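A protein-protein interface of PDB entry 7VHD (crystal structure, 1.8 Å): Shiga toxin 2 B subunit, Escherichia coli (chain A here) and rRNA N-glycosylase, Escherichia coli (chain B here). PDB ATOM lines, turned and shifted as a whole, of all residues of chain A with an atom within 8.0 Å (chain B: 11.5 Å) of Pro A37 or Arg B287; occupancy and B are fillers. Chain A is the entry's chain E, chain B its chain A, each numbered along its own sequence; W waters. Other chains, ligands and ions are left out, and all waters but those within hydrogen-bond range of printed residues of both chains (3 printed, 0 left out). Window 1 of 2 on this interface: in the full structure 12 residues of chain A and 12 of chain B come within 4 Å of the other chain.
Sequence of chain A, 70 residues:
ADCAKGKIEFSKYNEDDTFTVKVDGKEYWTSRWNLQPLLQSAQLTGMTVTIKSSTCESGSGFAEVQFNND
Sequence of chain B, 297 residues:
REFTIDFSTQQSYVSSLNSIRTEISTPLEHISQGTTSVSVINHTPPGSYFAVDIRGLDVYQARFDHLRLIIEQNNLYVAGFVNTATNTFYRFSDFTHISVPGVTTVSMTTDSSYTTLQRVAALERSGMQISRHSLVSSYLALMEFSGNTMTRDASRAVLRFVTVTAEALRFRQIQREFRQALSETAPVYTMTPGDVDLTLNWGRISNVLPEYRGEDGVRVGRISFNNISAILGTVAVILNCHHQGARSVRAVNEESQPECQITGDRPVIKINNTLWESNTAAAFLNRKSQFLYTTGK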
ATOM      1  N   PHE A  19      18.605  -5.937 -14.458  1.00  0.00           N
ATOM      2  CA  PHE A  19      20.060  -5.800 -14.416  1.00  0.00           C
ATOM      3  C   PHE A  19      20.558  -5.960 -15.843  1.00  0.00           C
ATOM      4  O   PHE A  19      20.449  -7.040 -16.422  1.00  0.00           O
ATOM      5  CB  PHE A  19      20.677  -6.840 -13.482  1.00  0.00           C
ATOM      6  CG  PHE A  19      22.133  -6.618 -13.173  1.00  0.00           C
ATOM      7  CD1 PHE A  19      22.524  -5.695 -12.212  1.00  0.00           C
ATOM      8  CD2 PHE A  19      23.105  -7.357 -13.816  1.00  0.00           C
ATOM      9  CE1 PHE A  19      23.860  -5.515 -11.914  1.00  0.00           C
ATOM     10  CE2 PHE A  19      24.450  -7.181 -13.519  1.00  0.00           C
ATOM     11  CZ  PHE A  19      24.823  -6.261 -12.569  1.00  0.00           C
ATOM     12  N   ARG A  32      17.144 -12.103 -12.563  1.00  0.00           N
ATOM     13  CA  ARG A  32      17.680 -13.078 -11.619  1.00  0.00           C
ATOM     14  C   ARG A  32      18.727 -12.400 -10.747  1.00  0.00           C
ATOM     15  O   ARG A  32      19.804 -12.031 -11.233  1.00  0.00           O
ATOM     16  CB  ARG A  32      18.285 -14.268 -12.363  1.00  0.00           C
ATOM     17  CG  ARG A  32      17.400 -14.831 -13.471  1.00  0.00           C
ATOM     18  CD  ARG A  32      16.170 -15.534 -12.893  1.00  0.00           C
ATOM     19  NE  ARG A  32      15.201 -15.831 -13.942  1.00  0.00           N
ATOM     20  CZ  ARG A  32      15.049 -17.022 -14.505  1.00  0.00           C
ATOM     21  NH1 ARG A  32      15.723 -18.075 -14.081  1.00  0.00           N
ATOM     22  NH2 ARG A  32      14.201 -17.156 -15.520  1.00  0.00           N
ATOM     23  N   TRP A  33      18.423 -12.222  -9.460  1.00  0.00           N
ATOM     24  CA  TRP A  33      19.423 -11.638  -8.581  1.00  0.00           C
ATOM     25  C   TRP A  33      20.632 -12.542  -8.464  1.00  0.00           C
ATOM     26  O   TRP A  33      21.740 -12.048  -8.245  1.00  0.00           O
ATOM     27  CB  TRP A  33      18.839 -11.353  -7.194  1.00  0.00           C
ATOM     28  CG  TRP A  33      18.098 -10.037  -7.098  1.00  0.00           C
ATOM     29  CD1 TRP A  33      17.455  -9.374  -8.106  1.00  0.00           C
ATOM     30  CD2 TRP A  33      17.910  -9.252  -5.912  1.00  0.00           C
ATOM     31  NE1 TRP A  33      16.879  -8.206  -7.616  1.00  0.00           N
ATOM     32  CE2 TRP A  33      17.145  -8.115  -6.273  1.00  0.00           C
ATOM     33  CE3 TRP A  33      18.315  -9.396  -4.585  1.00  0.00           C
ATOM     34  CZ2 TRP A  33      16.786  -7.125  -5.345  1.00  0.00           C
ATOM     35  CZ3 TRP A  33      17.955  -8.415  -3.667  1.00  0.00           C
ATOM     36  CH2 TRP A  33      17.194  -7.297  -4.052  1.00  0.00           C
ATOM     37  N   ASN A  34      20.443 -13.863  -8.598  1.00  0.00           N
ATOM     38  CA  ASN A  34      21.591 -14.767  -8.604  1.00  0.00           C
ATOM     39  C   ASN A  34      22.644 -14.283  -9.579  1.00  0.00           C
ATOM     40  O   ASN A  34      23.842 -14.430  -9.336  1.00  0.00           O
ATOM     41  CB  ASN A  34      21.186 -16.189  -9.010  1.00  0.00           C
ATOM     42  CG  ASN A  34      20.614 -17.002  -7.867  1.00  0.00           C
ATOM     43  OD1 ASN A  34      20.806 -16.685  -6.690  1.00  0.00           O
ATOM     44  ND2 ASN A  34      19.888 -18.058  -8.220  1.00  0.00           N
ATOM     45  N   LEU A  35      22.213 -13.722 -10.704  1.00  0.00           N
ATOM     46  CA  LEU A  35      23.168 -13.361 -11.738  1.00  0.00           C
ATOM     47  C   LEU A  35      23.872 -12.035 -11.468  1.00  0.00           C
ATOM     48  O   LEU A  35      24.891 -11.765 -12.105  1.00  0.00           O
ATOM     49  CB  LEU A  35      22.461 -13.324 -13.101  1.00  0.00           C
ATOM     50  CG  LEU A  35      22.394 -14.708 -13.746  1.00  0.00           C
ATOM     51  CD1 LEU A  35      21.480 -14.664 -14.963  1.00  0.00           C
ATOM     52  CD2 LEU A  35      23.801 -15.177 -14.130  1.00  0.00           C
ATOM     53  N   GLN A  36      23.389 -11.202 -10.540  1.00  0.00           N
ATOM     54  CA  GLN A  36      24.058  -9.913 -10.349  1.00  0.00           C
ATOM     55  C   GLN A  36      25.492 -10.061  -9.859  1.00  0.00           C
ATOM     56  O   GLN A  36      26.400  -9.508 -10.510  1.00  0.00           O
ATOM     57  CB  GLN A  36      23.220  -9.015  -9.436  1.00  0.00           C
ATOM     58  CG  GLN A  36      21.883  -8.684 -10.077  1.00  0.00           C
ATOM     59  CD  GLN A  36      21.152  -7.551  -9.391  1.00  0.00           C
ATOM     60  OE1 GLN A  36      21.743  -6.755  -8.651  1.00  0.00           O
ATOM     61  NE2 GLN A  36      19.849  -7.456  -9.660  1.00  0.00           N
ATOM     62  N   PRO A  37      25.783 -10.768  -8.760  1.00  0.00           N
ATOM     63  CA  PRO A  37      27.193 -10.898  -8.356  1.00  0.00           C
ATOM     64  C   PRO A  37      28.007 -11.697  -9.348  1.00  0.00           C
ATOM     65  O   PRO A  37      29.175 -11.371  -9.565  1.00  0.00           O
ATOM     66  CB  PRO A  37      27.117 -11.605  -6.998  1.00  0.00           C
ATOM     67  CG  PRO A  37      25.770 -12.268  -6.994  1.00  0.00           C
ATOM     68  CD  PRO A  37      24.876 -11.366  -7.764  1.00  0.00           C
ATOM     69  N   LEU A  38      27.409 -12.714  -9.973  1.00  0.00           N
ATOM     70  CA  LEU A  38      28.128 -13.506 -10.970  1.00  0.00           C
ATOM     71  C   LEU A  38      28.552 -12.637 -12.143  1.00  0.00           C
ATOM     72  O   LEU A  38      29.717 -12.652 -12.563  1.00  0.00           O
ATOM     73  CB  LEU A  38      27.250 -14.667 -11.447  1.00  0.00           C
ATOM     74  CG  LEU A  38      26.801 -15.622 -10.339  1.00  0.00           C
ATOM     75  CD1 LEU A  38      25.853 -16.690 -10.877  1.00  0.00           C
ATOM     76  CD2 LEU A  38      28.001 -16.262  -9.652  1.00  0.00           C
ATOM     77  N   LEU A  39      27.625 -11.824 -12.649  1.00  0.00           N
ATOM     78  CA  LEU A  39      27.930 -10.975 -13.790  1.00  0.00           C
ATOM     79  C   LEU A  39      28.890  -9.862 -13.409  1.00  0.00           C
ATOM     80  O   LEU A  39      29.786  -9.529 -14.183  1.00  0.00           O
ATOM     81  CB  LEU A  39      26.647 -10.391 -14.379  1.00  0.00           C
ATOM     82  CG  LEU A  39      25.760 -11.361 -15.165  1.00  0.00           C
ATOM     83  CD1 LEU A  39      24.412 -10.712 -15.403  1.00  0.00           C
ATOM     84  CD2 LEU A  39      26.429 -11.752 -16.497  1.00  0.00           C
ATOM     85  N   GLN A  40      28.709  -9.246 -12.239  1.00  0.00           N
ATOM     86  CA  GLN A  40      29.618  -8.166 -11.883  1.00  0.00           C
ATOM     87  C   GLN A  40      31.023  -8.688 -11.642  1.00  0.00           C
ATOM     88  O   GLN A  40      32.002  -8.039 -12.021  1.00  0.00           O
ATOM     89  CB  GLN A  40      29.122  -7.401 -10.659  1.00  0.00           C
ATOM     90  CG  GLN A  40      29.961  -6.128 -10.476  1.00  0.00           C
ATOM     91  CD  GLN A  40      29.964  -5.607  -9.057  1.00  0.00           C
ATOM     92  OE1 GLN A  40      30.112  -6.366  -8.098  1.00  0.00           O
ATOM     93  NE2 GLN A  40      29.796  -4.294  -8.919  1.00  0.00           N
ATOM     94  N   SER A  41      31.150  -9.851 -10.997  1.00  0.00           N
ATOM     95  CA  SER A  41      32.468 -10.453 -10.848  1.00  0.00           C
ATOM     96  C   SER A  41      33.077 -10.749 -12.209  1.00  0.00           C
ATOM     97  O   SER A  41      34.270 -10.499 -12.426  1.00  0.00           O
ATOM     98  CB  SER A  41      32.374 -11.726 -10.006  1.00  0.00           C
ATOM     99  OG  SER A  41      32.016 -11.404  -8.677  1.00  0.00           O
ATOM    100  N   ALA A  42      32.272 -11.280 -13.138  1.00  0.00           N
ATOM    101  CA  ALA A  42      32.765 -11.498 -14.500  1.00  0.00           C
ATOM    102  C   ALA A  42      33.261 -10.195 -15.116  1.00  0.00           C
ATOM    103  O   ALA A  42      34.310 -10.162 -15.771  1.00  0.00           O
ATOM    104  CB  ALA A  42      31.652 -12.111 -15.358  1.00  0.00           C
ATOM    105  N   GLN A  43      32.515  -9.107 -14.906  1.00  0.00           N
ATOM    106  CA  GLN A  43      32.905  -7.808 -15.443  1.00  0.00           C
ATOM    107  C   GLN A  43      34.236  -7.342 -14.865  1.00  0.00           C
ATOM    108  O   GLN A  43      35.145  -6.935 -15.602  1.00  0.00           O
ATOM    109  CB  GLN A  43      31.807  -6.779 -15.157  1.00  0.00           C
ATOM    110  CG  GLN A  43      32.157  -5.397 -15.682  1.00  0.00           C
ATOM    111  CD  GLN A  43      31.116  -4.377 -15.277  1.00  0.00           C
ATOM    112  OE1 GLN A  43      30.098  -4.731 -14.675  1.00  0.00           O
ATOM    113  NE2 GLN A  43      31.345  -3.119 -15.627  1.00  0.00           N
ATOM    114  N   LEU A  44      34.373  -7.388 -13.541  1.00  0.00           N
ATOM    115  CA  LEU A  44      35.554  -6.802 -12.929  1.00  0.00           C
ATOM    116  C   LEU A  44      36.791  -7.671 -13.085  1.00  0.00           C
ATOM    117  O   LEU A  44      37.905  -7.156 -12.939  1.00  0.00           O
ATOM    118  CB  LEU A  44      35.289  -6.496 -11.452  1.00  0.00           C
ATOM    119  CG  LEU A  44      35.108  -7.590 -10.403  1.00  0.00           C
ATOM    120  CD1 LEU A  44      36.440  -7.859  -9.717  1.00  0.00           C
ATOM    121  CD2 LEU A  44      34.060  -7.137  -9.387  1.00  0.00           C
ATOM    122  N   PHE A  67      30.332 -18.543 -18.418  1.00  0.00           N
ATOM    123  CA  PHE A  67      31.474 -17.804 -17.906  1.00  0.00           C
ATOM    124  C   PHE A  67      32.743 -18.585 -18.221  1.00  0.00           C
ATOM    125  O   PHE A  67      32.852 -19.763 -17.846  1.00  0.00           O
ATOM    126  CB  PHE A  67      31.364 -17.627 -16.384  1.00  0.00           C
ATOM    127  CG  PHE A  67      30.130 -16.908 -15.949  1.00  0.00           C
ATOM    128  CD1 PHE A  67      28.955 -17.610 -15.712  1.00  0.00           C
ATOM    129  CD2 PHE A  67      30.137 -15.531 -15.788  1.00  0.00           C
ATOM    130  CE1 PHE A  67      27.803 -16.957 -15.320  1.00  0.00           C
ATOM    131  CE2 PHE A  67      28.982 -14.868 -15.381  1.00  0.00           C
ATOM    132  CZ  PHE A  67      27.814 -15.584 -15.154  1.00  0.00           C
ATOM    133  N   ASN B 279      42.671  -6.045  -4.351  1.00  0.00           N
ATOM    134  CA  ASN B 279      41.336  -5.466  -4.446  1.00  0.00           C
ATOM    135  C   ASN B 279      40.450  -6.233  -5.425  1.00  0.00           C
ATOM    136  O   ASN B 279      39.233  -6.307  -5.226  1.00  0.00           O
ATOM    137  CB  ASN B 279      41.442  -3.991  -4.834  1.00  0.00           C
ATOM    138  CG  ASN B 279      41.690  -3.097  -3.627  1.00  0.00           C
ATOM    139  OD1 ASN B 279      41.343  -3.458  -2.499  1.00  0.00           O
ATOM    140  ND2 ASN B 279      42.295  -1.938  -3.852  1.00  0.00           N
ATOM    141  N   THR B 280      41.031  -6.848  -6.460  1.00  0.00           N
ATOM    142  CA  THR B 280      40.226  -7.663  -7.372  1.00  0.00           C
ATOM    143  C   THR B 280      39.662  -8.890  -6.654  1.00  0.00           C
ATOM    144  O   THR B 280      38.455  -9.203  -6.745  1.00  0.00           O
ATOM    145  CB  THR B 280      41.069  -8.081  -8.584  1.00  0.00           C
ATOM    146  OG1 THR B 280      41.457  -6.917  -9.331  1.00  0.00           O
ATOM    147  CG2 THR B 280      40.307  -9.033  -9.494  1.00  0.00           C
ATOM    148  N   ALA B 281      40.529  -9.602  -5.929  1.00  0.00           N
ATOM    149  CA  ALA B 281      40.063 -10.758  -5.170  1.00  0.00           C
ATOM    150  C   ALA B 281      39.012 -10.332  -4.156  1.00  0.00           C
ATOM    151  O   ALA B 281      37.947 -10.955  -4.048  1.00  0.00           O
ATOM    152  CB  ALA B 281      41.241 -11.446  -4.481  1.00  0.00           C
ATOM    153  N   ALA B 282      39.284  -9.242  -3.428  1.00  0.00           N
ATOM    154  CA  ALA B 282      38.324  -8.744  -2.446  1.00  0.00           C
ATOM    155  C   ALA B 282      36.976  -8.476  -3.088  1.00  0.00           C
ATOM    156  O   ALA B 282      35.929  -8.702  -2.471  1.00  0.00           O
ATOM    157  CB  ALA B 282      38.858  -7.465  -1.792  1.00  0.00           C
ATOM    158  N   ALA B 283      36.983  -7.983  -4.329  1.00  0.00           N
ATOM    159  CA  ALA B 283      35.754  -7.582  -4.990  1.00  0.00           C
ATOM    160  C   ALA B 283      34.930  -8.750  -5.499  1.00  0.00           C
ATOM    161  O   ALA B 283      33.765  -8.539  -5.859  1.00  0.00           O
ATOM    162  CB  ALA B 283      36.069  -6.633  -6.153  1.00  0.00           C
ATOM    163  N   PHE B 284      35.492  -9.960  -5.582  1.00  0.00           N
ATOM    164  CA  PHE B 284      34.598 -11.106  -5.771  1.00  0.00           C
ATOM    165  C   PHE B 284      34.504 -12.046  -4.567  1.00  0.00           C
ATOM    166  O   PHE B 284      33.774 -13.042  -4.633  1.00  0.00           O
ATOM    167  CB  PHE B 284      34.932 -11.877  -7.056  1.00  0.00           C
ATOM    168  CG  PHE B 284      36.271 -12.557  -7.077  1.00  0.00           C
ATOM    169  CD1 PHE B 284      36.443 -13.807  -6.500  1.00  0.00           C
ATOM    170  CD2 PHE B 284      37.328 -11.994  -7.780  1.00  0.00           C
ATOM    171  CE1 PHE B 284      37.673 -14.474  -6.571  1.00  0.00           C
ATOM    172  CE2 PHE B 284      38.565 -12.648  -7.862  1.00  0.00           C
ATOM    173  CZ  PHE B 284      38.745 -13.879  -7.255  1.00  0.00           C
ATOM    174  N   LEU B 285      35.156 -11.727  -3.448  1.00  0.00           N
ATOM    175  CA  LEU B 285      35.045 -12.513  -2.225  1.00  0.00           C
ATOM    176  C   LEU B 285      34.222 -11.799  -1.158  1.00  0.00           C
ATOM    177  O   LEU B 285      34.318 -12.134   0.026  1.00  0.00           O
ATOM    178  CB  LEU B 285      36.441 -12.841  -1.691  1.00  0.00           C
ATOM    179  CG  LEU B 285      37.321 -13.665  -2.641  1.00  0.00           C
ATOM    180  CD1 LEU B 285      38.733 -13.772  -2.095  1.00  0.00           C
ATOM    181  CD2 LEU B 285      36.706 -15.064  -2.862  1.00  0.00           C
ATOM    182  N   ASN B 286      33.437 -10.796  -1.545  1.00  0.00           N
ATOM    183  CA  ASN B 286      32.630 -10.033  -0.604  1.00  0.00           C
ATOM    184  C   ASN B 286      31.145 -10.353  -0.735  1.00  0.00           C
ATOM    185  O   ASN B 286      30.309  -9.556  -0.303  1.00  0.00           O
ATOM    186  CB  ASN B 286      32.866  -8.533  -0.783  1.00  0.00           C
ATOM    187  CG  ASN B 286      32.369  -8.026  -2.110  1.00  0.00           C
ATOM    188  OD1 ASN B 286      32.077  -8.810  -3.015  1.00  0.00           O
ATOM    189  ND2 ASN B 286      32.275  -6.708  -2.246  1.00  0.00           N
ATOM    190  N   ARG B 287      30.806 -11.505  -1.314  1.00  0.00           N
ATOM    191  CA  ARG B 287      29.419 -11.909  -1.486  1.00  0.00           C
ATOM    192  C   ARG B 287      28.976 -12.746  -0.290  1.00  0.00           C
ATOM    193  O   ARG B 287      29.739 -13.570   0.218  1.00  0.00           O
ATOM    194  CB  ARG B 287      29.264 -12.722  -2.769  1.00  0.00           C
ATOM    195  CG  ARG B 287      29.196 -11.906  -4.059  1.00  0.00           C
ATOM    196  CD  ARG B 287      30.565 -11.370  -4.495  1.00  0.00           C
ATOM    197  NE  ARG B 287      30.488 -10.869  -5.862  1.00  0.00           N
ATOM    198  CZ  ARG B 287      30.450  -9.581  -6.179  1.00  0.00           C
ATOM    199  NH1 ARG B 287      30.506  -8.640  -5.252  1.00  0.00           N
ATOM    200  NH2 ARG B 287      30.326  -9.227  -7.461  1.00  0.00           N
ATOM    201  N   LYS B 288      27.739 -12.543   0.159  1.00  0.00           N
ATOM    202  CA  LYS B 288      27.220 -13.421   1.195  1.00  0.00           C
ATOM    203  C   LYS B 288      26.625 -14.673   0.556  1.00  0.00           C
ATOM    204  O   LYS B 288      26.706 -14.888  -0.658  1.00  0.00           O
ATOM    205  CB  LYS B 288      26.191 -12.708   2.069  1.00  0.00           C
ATOM    206  CG  LYS B 288      24.835 -12.510   1.435  1.00  0.00           C
ATOM    207  CD  LYS B 288      23.923 -11.757   2.435  1.00  0.00           C
ATOM    208  CE  LYS B 288      22.560 -11.428   1.848  1.00  0.00           C
ATOM    209  NZ  LYS B 288      21.660 -10.816   2.866  1.00  0.00           N
ATOM    210  N   SER B 289      26.036 -15.521   1.389  1.00  0.00           N
ATOM    211  CA  SER B 289      25.401 -16.736   0.891  1.00  0.00           C
ATOM    212  C   SER B 289      24.403 -16.411  -0.210  1.00  0.00           C
ATOM    213  O   SER B 289      23.533 -15.557  -0.042  1.00  0.00           O
ATOM    214  CB  SER B 289      24.700 -17.457   2.041  1.00  0.00           C
ATOM    215  OG  SER B 289      23.923 -18.527   1.540  1.00  0.00           O
ATOM    216  N   GLN B 290      24.522 -17.119  -1.329  1.00  0.00           N
ATOM    217  CA  GLN B 290      23.741 -16.780  -2.519  1.00  0.00           C
ATOM    218  C   GLN B 290      22.238 -16.901  -2.271  1.00  0.00           C
ATOM    219  O   GLN B 290      21.461 -16.042  -2.706  1.00  0.00           O
ATOM    220  CB  GLN B 290      24.157 -17.680  -3.678  1.00  0.00           C
ATOM    221  CG  GLN B 290      23.472 -17.381  -5.007  1.00  0.00           C
ATOM    222  CD  GLN B 290      24.144 -16.272  -5.789  1.00  0.00           C
ATOM    223  OE1 GLN B 290      24.565 -15.256  -5.221  1.00  0.00           O
ATOM    224  NE2 GLN B 290      24.216 -16.441  -7.112  1.00  0.00           N
ATOM    225  N   PHE B 291      21.800 -17.988  -1.623  1.00  0.00           N
ATOM    226  CA  PHE B 291      20.367 -18.157  -1.371  1.00  0.00           C
ATOM    227  C   PHE B 291      19.814 -16.991  -0.548  1.00  0.00           C
ATOM    228  O   PHE B 291      18.742 -16.441  -0.854  1.00  0.00           O
ATOM    229  CB  PHE B 291      20.110 -19.489  -0.653  1.00  0.00           C
ATOM    230  CG  PHE B 291      18.649 -19.848  -0.529  1.00  0.00           C
ATOM    231  CD1 PHE B 291      18.009 -20.585  -1.516  1.00  0.00           C
ATOM    232  CD2 PHE B 291      17.916 -19.443   0.578  1.00  0.00           C
ATOM    233  CE1 PHE B 291      16.665 -20.914  -1.395  1.00  0.00           C
ATOM    234  CE2 PHE B 291      16.557 -19.780   0.699  1.00  0.00           C
ATOM    235  CZ  PHE B 291      15.948 -20.504  -0.288  1.00  0.00           C
ATOM    236  N   LEU B 292      20.556 -16.582   0.484  1.00  0.00           N
ATOM    237  CA  LEU B 292      20.137 -15.458   1.321  1.00  0.00           C
ATOM    238  C   LEU B 292      20.142 -14.152   0.537  1.00  0.00           C
ATOM    239  O   LEU B 292      19.250 -13.309   0.711  1.00  0.00           O
ATOM    240  CB  LEU B 292      21.065 -15.349   2.525  1.00  0.00           C
ATOM    241  CG  LEU B 292      21.223 -16.645   3.321  1.00  0.00           C
ATOM    242  CD1 LEU B 292      22.087 -16.408   4.556  1.00  0.00           C
ATOM    243  CD2 LEU B 292      19.835 -17.226   3.692  1.00  0.00           C
ATOM    244  N   TYR B 293      21.148 -13.969  -0.322  1.00  0.00           N
ATOM    245  CA  TYR B 293      21.222 -12.766  -1.145  1.00  0.00           C
ATOM    246  C   TYR B 293      20.001 -12.644  -2.040  1.00  0.00           C
ATOM    247  O   TYR B 293      19.330 -11.600  -2.083  1.00  0.00           O
ATOM    248  CB  TYR B 293      22.477 -12.819  -2.008  1.00  0.00           C
ATOM    249  CG  TYR B 293      22.614 -11.676  -2.995  1.00  0.00           C
ATOM    250  CD1 TYR B 293      23.046 -10.429  -2.576  1.00  0.00           C
ATOM    251  CD2 TYR B 293      22.365 -11.866  -4.356  1.00  0.00           C
ATOM    252  CE1 TYR B 293      23.205  -9.379  -3.484  1.00  0.00           C
ATOM    253  CE2 TYR B 293      22.536 -10.824  -5.272  1.00  0.00           C
ATOM    254  CZ  TYR B 293      22.954  -9.588  -4.825  1.00  0.00           C
ATOM    255  OH  TYR B 293      23.132  -8.545  -5.715  1.00  0.00           O
ATOM    256  N   THR B 294      19.712 -13.705  -2.780  1.00  0.00           N
ATOM    257  CA  THR B 294      18.689 -13.618  -3.808  1.00  0.00           C
ATOM    258  C   THR B 294      17.291 -13.573  -3.210  1.00  0.00           C
ATOM    259  O   THR B 294      16.413 -12.893  -3.757  1.00  0.00           O
ATOM    260  CB  THR B 294      18.871 -14.778  -4.783  1.00  0.00           C
ATOM    261  OG1 THR B 294      20.100 -14.576  -5.487  1.00  0.00           O
ATOM    262  CG2 THR B 294      17.702 -14.883  -5.767  1.00  0.00           C
ATOM    263  N   THR B 295      17.066 -14.237  -2.076  1.00  0.00           N
ATOM    264  CA  THR B 295      15.733 -14.203  -1.495  1.00  0.00           C
ATOM    265  C   THR B 295      15.522 -13.010  -0.574  1.00  0.00           C
ATOM    266  O   THR B 295      14.369 -12.696  -0.255  1.00  0.00           O
ATOM    267  CB  THR B 295      15.439 -15.498  -0.733  1.00  0.00           C
ATOM    268  OG1 THR B 295      16.306 -15.596   0.400  1.00  0.00           O
ATOM    269  CG2 THR B 295      15.675 -16.712  -1.656  1.00  0.00           C
ATOM    270  N   GLY B 296      16.592 -12.319  -0.165  1.00  0.00           N
ATOM    271  CA  GLY B 296      16.411 -11.168   0.695  1.00  0.00           C
ATOM    272  C   GLY B 296      16.221  -9.891  -0.090  1.00  0.00           C
ATOM    273  O   GLY B 296      17.096  -9.018  -0.089  1.00  0.00           O
ATOM    274  N   LYS B 297      15.078  -9.774  -0.760  1.00  0.00           N
ATOM    275  CA  LYS B 297      14.830  -8.658  -1.672  1.00  0.00           C
ATOM    276  C   LYS B 297      14.245  -7.438  -0.975  1.00  0.00           C
ATOM    277  O   LYS B 297      13.811  -7.495   0.179  1.00  0.00           O
ATOM    278  CB  LYS B 297      13.894  -9.104  -2.782  1.00  0.00           C
ATOM    279  CG  LYS B 297      14.494 -10.199  -3.674  1.00  0.00           C
ATOM    280  CD  LYS B 297      13.637 -10.392  -4.923  1.00  0.00           C
ATOM    281  CE  LYS B 297      14.050 -11.638  -5.699  1.00  0.00           C
ATOM    282  NZ  LYS B 297      15.469 -11.534  -6.173  1.00  0.00           N
ATOM    283  OXT LYS B 297      14.202  -6.365  -1.577  1.00  0.00           O
HETATM  284  O   HOH W   1      15.853 -13.188  -8.532  1.00  0.00           O
HETATM  285  O   HOH W   2      14.300  -9.837  -8.673  1.00  0.00           O
HETATM  286  O   HOH W   3      30.842 -13.646  -7.385  1.00  0.00           O
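The backbone carbonyl oxygen (O) of Pro A37 sits at hydrogen-bond distance from the guanidinium group (NH2) of Arg B287 (3.2 Å).
NH2 of Arg B287 sits at hydrogen-bond distance from OE1 of Gln A40 (2.9 Å).
The guanidinium group (NH2) of Arg B287 lies within hydrogen-bond range of the side-chain hydroxyl (OG) of Ser A41 (3.0 Å).
The side-chain amide nitrogen of Gln B290 is in hydrogen-bond range of the backbone carbonyl oxygen of Asn A34, at 3.0 Å.
The side-chain hydroxyl (OG1) of Thr B294 sits at hydrogen-bond distance from the side-chain amide oxygen (OD1) of Asn A34 (2.5 Å).
OD1 of Asn B286 sits close to O of Ala B283, 3.3 Å away.
NH1 of Arg B287 sits at hydrogen-bond distance from O of Ala B283 (3.3 Å).
The guanidinium group of Arg B287 is in hydrogen-bond range of the side-chain amide oxygen of Asn B286.
O of Gln B290 is in hydrogen-bond range of OG1 of Thr B294, at 3.4 Å.
O of Thr B294 is in hydrogen-bond range of NZ of Lys B297 (2.9 Å).
O of Pro A37 is in hydrogen-bond range of OG of Ser A41, at 3.0 Å.
Among the printed residues, merely in contact across the chains: Trp A33 with Lys B297 (3.2 Å), Trp A33 with Tyr B293 (3.3 Å), Ser A41 with Phe B284 (3.4 Å), Pro A37 with Tyr B293 (3.5 Å), Trp A33 with Thr B294 (3.6 Å), Pro A37 with Gln B290 (3.7 Å), Gln A36 with Tyr B293 (3.7 Å), Trp A33 with Gly B296 (3.7 Å), Leu A44 with Ala B283 (3.8 Å) and Leu A44 with Thr B280 (3.8 Å).
Pro A37 touches just these residues of chain B: Arg B287 (3.2 Å), Gln B290 (3.7 Å) and Tyr B293 (3.5 Å).
Arg B287 touches just these residues of chain A: Pro A37, Gln A40 and Ser A41.
No residue of chain B comes within 4 Å of Leu A38.
Gln A40 touches one residue of chain B.
Of chain B, only Phe B284 and Arg B287 come within 4 Å of Ser A41.
Of the printed residues of chain A, Thr B280 touches Leu A44 (3.8 Å).
Printed residues of chain A within 4 Å of Lys B297: Trp A33.
Printed residues of chain B within 4 Å of Trp A33: Tyr B293, Thr B294, Gly B296 and Lys B297.
Asn B286 touches none of the printed residues of chain A.
The nearest residue of chain B that does not touch Pro A37 is Thr B294 (6.2 Å).
The nearest printed residue of chain A that does not touch Gln B290 is Leu A38 (4.1 Å).
Of the 19 printed residues of chain B, 9 touch a printed residue of chain A.
Printed residues of chain B that touch a printed residue of chain A: Thr B280, Ala B283, Phe B284, Arg B287, Gln B290, Tyr B293, Thr B294, Gly B296 and Lys B297.
Among the printed residues, no Asp or Glu carboxylate lies within 4 Å of a Lys or Arg side-chain nitrogen of the other chain.
Water W3 bridges the side-chain hydroxyl of Ser A41 (2.8 Å) and the guanidinium group of Arg B287 (3.2 Å).
Water W1 lies within hydrogen-bond range of N of Trp A33 and NZ of Lys B297.
Water W2 lies within hydrogen-bond range of the indole nitrogen (NE1) of Trp A33 (3.2 Å) and the side-chain amino group (NZ) of Lys B297 (3.2 Å).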
